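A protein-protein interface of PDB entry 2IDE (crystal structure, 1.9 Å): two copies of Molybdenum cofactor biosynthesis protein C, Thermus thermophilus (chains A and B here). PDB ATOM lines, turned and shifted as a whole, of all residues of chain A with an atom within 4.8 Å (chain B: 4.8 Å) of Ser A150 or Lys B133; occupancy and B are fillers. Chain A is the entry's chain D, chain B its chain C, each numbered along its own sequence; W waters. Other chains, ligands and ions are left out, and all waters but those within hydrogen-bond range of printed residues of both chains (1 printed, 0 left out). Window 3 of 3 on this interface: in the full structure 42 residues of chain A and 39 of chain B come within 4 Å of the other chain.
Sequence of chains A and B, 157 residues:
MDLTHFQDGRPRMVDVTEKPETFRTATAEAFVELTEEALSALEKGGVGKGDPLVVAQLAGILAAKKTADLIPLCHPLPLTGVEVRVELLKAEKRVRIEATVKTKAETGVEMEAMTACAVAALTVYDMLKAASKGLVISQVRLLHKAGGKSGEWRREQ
Of chain B, only Lys B133 comes within 4 Å of Ser A150.
Lys B133 touches four residues of chain A.
Of the printed residues of chain B, Trp A153 touches Lys B133 (3.6 Å) and Gly B134 (3.9 Å).
Of the printed residues of chain A, Gly B134 touches Trp A153.
Printed residues of chain B within 4 Å of Leu A142: Tyr B125 and Lys B133.
Glu A152 touches none of the printed residues of chain B.
The nearest printed residue of chain B that does not touch Ser A150 is Ala B130 (6.1 Å).
The nearest printed residue of chain A that does not touch Gly B134 is Leu A142 (5.8 Å).
The side-chain hydroxyl (OH) of Tyr B125 lies within hydrogen-bond range of the backbone carbonyl oxygen (O) of Lys B133 (2.8 Å).
O of Lys A145 lies within hydrogen-bond range of N of Trp A153, 2.8 Å away.
Of the 8 printed residues of chain B, 3 touch a printed residue of chain A.
Printed residues of chain B that touch a printed residue of chain A: Tyr B125, Lys B133 and Gly B134.
Hydrophobic or aromatic side chains of chain B that line the printed part of chain A: Tyr B125.
Hydrophobic or aromatic side chains of chain A that line the printed part of chain B: Leu A142 and Trp A153.
Among the printed residues, 6 pairs touch across the chains.
No position is printed for both chains.
Water W1 lies within hydrogen-bond range of the backbone carbonyl oxygen of Leu B135, the backbone carbonyl oxygen of Lys B133 and the backbone NH of Leu A142.
CD2 of Leu A142 touches OH of Tyr B125 (3.6 Å).
Leu A142 touches Lys B133 (CB to O, 3.95 Å).
NZ of Lys A145 touches CG of Lys B133, at 3.3 Å.
Ser A150 touches Lys B133 (CB to CE, 3.9 Å).
CD of Lys B133 touches CD1 of Trp A153, at 3.6 Å.
Gly B134 touches Trp A153.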
ATOM      1  N   LEU A 142      21.244  14.159 -17.907  1.00  0.00           N
ATOM      2  CA  LEU A 142      20.357  14.055 -16.759  1.00  0.00           C
ATOM      3  C   LEU A 142      19.456  15.288 -16.708  1.00  0.00           C
ATOM      4  O   LEU A 142      19.899  16.397 -16.981  1.00  0.00           O
ATOM      5  CB  LEU A 142      21.183  13.948 -15.473  1.00  0.00           C
ATOM      6  CG  LEU A 142      20.413  13.537 -14.214  1.00  0.00           C
ATOM      7  CD1 LEU A 142      19.996  12.086 -14.335  1.00  0.00           C
ATOM      8  CD2 LEU A 142      21.286  13.728 -12.981  1.00  0.00           C
ATOM      9  N   LYS A 145      17.060  14.855 -10.460  1.00  0.00           N
ATOM     10  CA  LYS A 145      17.444  13.847  -9.489  1.00  0.00           C
ATOM     11  C   LYS A 145      17.225  14.426  -8.099  1.00  0.00           C
ATOM     12  O   LYS A 145      17.359  15.634  -7.894  1.00  0.00           O
ATOM     13  CB  LYS A 145      18.907  13.434  -9.660  1.00  0.00           C
ATOM     14  CG  LYS A 145      19.921  14.386  -9.057  1.00  0.00           C
ATOM     15  CD  LYS A 145      21.298  13.747  -9.057  1.00  0.00           C
ATOM     16  CE  LYS A 145      22.301  14.574  -8.274  1.00  0.00           C
ATOM     17  NZ  LYS A 145      23.618  13.880  -8.173  1.00  0.00           N
ATOM     18  N   GLY A 148      19.664  12.517  -2.750  1.00  0.00           N
ATOM     19  CA  GLY A 148      21.045  12.411  -2.314  1.00  0.00           C
ATOM     20  C   GLY A 148      21.451  13.483  -1.316  1.00  0.00           C
ATOM     21  O   GLY A 148      20.640  14.324  -0.927  1.00  0.00           O
ATOM     22  N   LYS A 149      22.712  13.446  -0.902  1.00  0.00           N
ATOM     23  CA  LYS A 149      23.236  14.420   0.046  1.00  0.00           C
ATOM     24  C   LYS A 149      23.203  15.804  -0.597  1.00  0.00           C
ATOM     25  O   LYS A 149      22.947  16.804   0.071  1.00  0.00           O
ATOM     26  CB  LYS A 149      24.671  14.051   0.435  1.00  0.00           C
ATOM     27  CG  LYS A 149      25.290  14.938   1.508  1.00  0.00           C
ATOM     28  CD  LYS A 149      26.711  14.495   1.829  1.00  0.00           C
ATOM     29  CE  LYS A 149      27.365  15.409   2.856  1.00  0.00           C
ATOM     30  NZ  LYS A 149      26.658  15.388   4.167  1.00  0.00           N
ATOM     31  N   SER A 150      23.452  15.848  -1.902  1.00  0.00           N
ATOM     32  CA  SER A 150      23.453  17.102  -2.648  1.00  0.00           C
ATOM     33  C   SER A 150      22.038  17.650  -2.815  1.00  0.00           C
ATOM     34  O   SER A 150      21.849  18.783  -3.259  1.00  0.00           O
ATOM     35  CB  SER A 150      24.090  16.892  -4.024  1.00  0.00           C
ATOM     36  OG  SER A 150      25.431  16.451  -3.901  1.00  0.00           O
ATOM     37  N   GLY A 151      21.050  16.834  -2.464  1.00  0.00           N
ATOM     38  CA  GLY A 151      19.664  17.250  -2.567  1.00  0.00           C
ATOM     39  C   GLY A 151      19.097  17.268  -3.973  1.00  0.00           C
ATOM     40  O   GLY A 151      19.615  16.611  -4.879  1.00  0.00           O
ATOM     41  N   GLU A 152      18.020  18.030  -4.146  1.00  0.00           N
ATOM     42  CA  GLU A 152      17.347  18.158  -5.432  1.00  0.00           C
ATOM     43  C   GLU A 152      18.215  18.816  -6.490  1.00  0.00           C
ATOM     44  O   GLU A 152      18.975  19.740  -6.199  1.00  0.00           O
ATOM     45  CB  GLU A 152      16.054  18.959  -5.269  1.00  0.00           C
ATOM     46  CG  GLU A 152      14.809  18.103  -5.169  1.00  0.00           C
ATOM     47  CD  GLU A 152      13.833  18.375  -6.297  1.00  0.00           C
ATOM     48  OE1 GLU A 152      12.867  17.598  -6.453  1.00  0.00           O
ATOM     49  OE2 GLU A 152      14.029  19.369  -7.026  1.00  0.00           O
ATOM     50  N   TRP A 153      18.086  18.339  -7.725  1.00  0.00           N
ATOM     51  CA  TRP A 153      18.853  18.874  -8.842  1.00  0.00           C
ATOM     52  C   TRP A 153      18.034  18.813 -10.130  1.00  0.00           C
ATOM     53  O   TRP A 153      17.372  17.816 -10.409  1.00  0.00           O
ATOM     54  CB  TRP A 153      20.142  18.075  -9.029  1.00  0.00           C
ATOM     55  CG  TRP A 153      21.039  18.633 -10.095  1.00  0.00           C
ATOM     56  CD1 TRP A 153      22.014  19.576  -9.936  1.00  0.00           C
ATOM     57  CD2 TRP A 153      21.011  18.316 -11.493  1.00  0.00           C
ATOM     58  NE1 TRP A 153      22.593  19.869 -11.148  1.00  0.00           N
ATOM     59  CE2 TRP A 153      21.996  19.109 -12.122  1.00  0.00           C
ATOM     60  CE3 TRP A 153      20.248  17.441 -12.277  1.00  0.00           C
ATOM     61  CZ2 TRP A 153      22.239  19.056 -13.498  1.00  0.00           C
ATOM     62  CZ3 TRP A 153      20.489  17.388 -13.649  1.00  0.00           C
ATOM     63  CH2 TRP A 153      21.477  18.191 -14.242  1.00  0.00           C
ATOM     64  N   TYR B 125      30.887   9.282 -17.290  1.00  0.00           N
ATOM     65  CA  TYR B 125      29.894  10.046 -16.548  1.00  0.00           C
ATOM     66  C   TYR B 125      29.813   9.536 -15.111  1.00  0.00           C
ATOM     67  O   TYR B 125      29.806  10.318 -14.163  1.00  0.00           O
ATOM     68  CB  TYR B 125      28.517   9.920 -17.211  1.00  0.00           C
ATOM     69  CG  TYR B 125      27.428  10.698 -16.501  1.00  0.00           C
ATOM     70  CD1 TYR B 125      27.277  12.075 -16.700  1.00  0.00           C
ATOM     71  CD2 TYR B 125      26.574  10.067 -15.600  1.00  0.00           C
ATOM     72  CE1 TYR B 125      26.303  12.799 -16.011  1.00  0.00           C
ATOM     73  CE2 TYR B 125      25.599  10.780 -14.906  1.00  0.00           C
ATOM     74  CZ  TYR B 125      25.470  12.147 -15.115  1.00  0.00           C
ATOM     75  OH  TYR B 125      24.522  12.850 -14.413  1.00  0.00           O
ATOM     76  N   LYS B 129      30.547  11.899 -12.154  1.00  0.00           N
ATOM     77  CA  LYS B 129      29.211  12.290 -11.728  1.00  0.00           C
ATOM     78  C   LYS B 129      29.247  13.150 -10.459  1.00  0.00           C
ATOM     79  O   LYS B 129      28.516  14.138 -10.343  1.00  0.00           O
ATOM     80  CB  LYS B 129      28.385  11.019 -11.489  1.00  0.00           C
ATOM     81  CG  LYS B 129      26.896  11.235 -11.323  1.00  0.00           C
ATOM     82  CD  LYS B 129      26.117   9.928 -11.439  1.00  0.00           C
ATOM     83  CE  LYS B 129      26.311   9.006 -10.240  1.00  0.00           C
ATOM     84  NZ  LYS B 129      27.662   8.386 -10.169  1.00  0.00           N
ATOM     85  N   ALA B 130      30.113  12.774  -9.521  1.00  0.00           N
ATOM     86  CA  ALA B 130      30.246  13.484  -8.251  1.00  0.00           C
ATOM     87  C   ALA B 130      30.641  14.948  -8.417  1.00  0.00           C
ATOM     88  O   ALA B 130      30.143  15.815  -7.699  1.00  0.00           O
ATOM     89  CB  ALA B 130      31.261  12.773  -7.369  1.00  0.00           C
ATOM     90  N   ALA B 131      31.534  15.222  -9.360  1.00  0.00           N
ATOM     91  CA  ALA B 131      31.991  16.584  -9.600  1.00  0.00           C
ATOM     92  C   ALA B 131      30.991  17.417 -10.403  1.00  0.00           C
ATOM     93  O   ALA B 131      30.877  18.624 -10.191  1.00  0.00           O
ATOM     94  CB  ALA B 131      33.345  16.562 -10.313  1.00  0.00           C
ATOM     95  N   SER B 132      30.272  16.777 -11.324  1.00  0.00           N
ATOM     96  CA  SER B 132      29.295  17.479 -12.157  1.00  0.00           C
ATOM     97  C   SER B 132      28.181  16.563 -12.645  1.00  0.00           C
ATOM     98  O   SER B 132      28.419  15.648 -13.431  1.00  0.00           O
ATOM     99  CB  SER B 132      29.986  18.108 -13.369  1.00  0.00           C
ATOM    100  OG  SER B 132      30.925  19.093 -12.974  1.00  0.00           O
ATOM    101  N   LYS B 133      26.965  16.828 -12.186  1.00  0.00           N
ATOM    102  CA  LYS B 133      25.802  16.036 -12.567  1.00  0.00           C
ATOM    103  C   LYS B 133      25.337  16.391 -13.979  1.00  0.00           C
ATOM    104  O   LYS B 133      24.682  15.587 -14.647  1.00  0.00           O
ATOM    105  CB  LYS B 133      24.668  16.287 -11.571  1.00  0.00           C
ATOM    106  CG  LYS B 133      25.081  16.073 -10.122  1.00  0.00           C
ATOM    107  CD  LYS B 133      24.501  17.141  -9.205  1.00  0.00           C
ATOM    108  CE  LYS B 133      25.099  17.045  -7.805  1.00  0.00           C
ATOM    109  NZ  LYS B 133      26.581  17.217  -7.813  1.00  0.00           N
ATOM    110  N   GLY B 134      25.700  17.590 -14.431  1.00  0.00           N
ATOM    111  CA  GLY B 134      25.288  18.054 -15.746  1.00  0.00           C
ATOM    112  C   GLY B 134      26.153  17.681 -16.934  1.00  0.00           C
ATOM    113  O   GLY B 134      25.981  18.242 -18.018  1.00  0.00           O
ATOM    114  N   LEU B 135      27.089  16.756 -16.753  1.00  0.00           N
ATOM    115  CA  LEU B 135      27.932  16.344 -17.863  1.00  0.00           C
ATOM    116  C   LEU B 135      27.035  15.729 -18.922  1.00  0.00           C
ATOM    117  O   LEU B 135      26.078  15.018 -18.606  1.00  0.00           O
ATOM    118  CB  LEU B 135      28.978  15.321 -17.419  1.00  0.00           C
ATOM    119  CG  LEU B 135      30.094  15.823 -16.505  1.00  0.00           C
ATOM    120  CD1 LEU B 135      31.086  14.697 -16.265  1.00  0.00           C
ATOM    121  CD2 LEU B 135      30.795  17.019 -17.143  1.00  0.00           C
HETATM  122  O   HOH W   1      23.839  15.324 -17.288  1.00  0.00           O
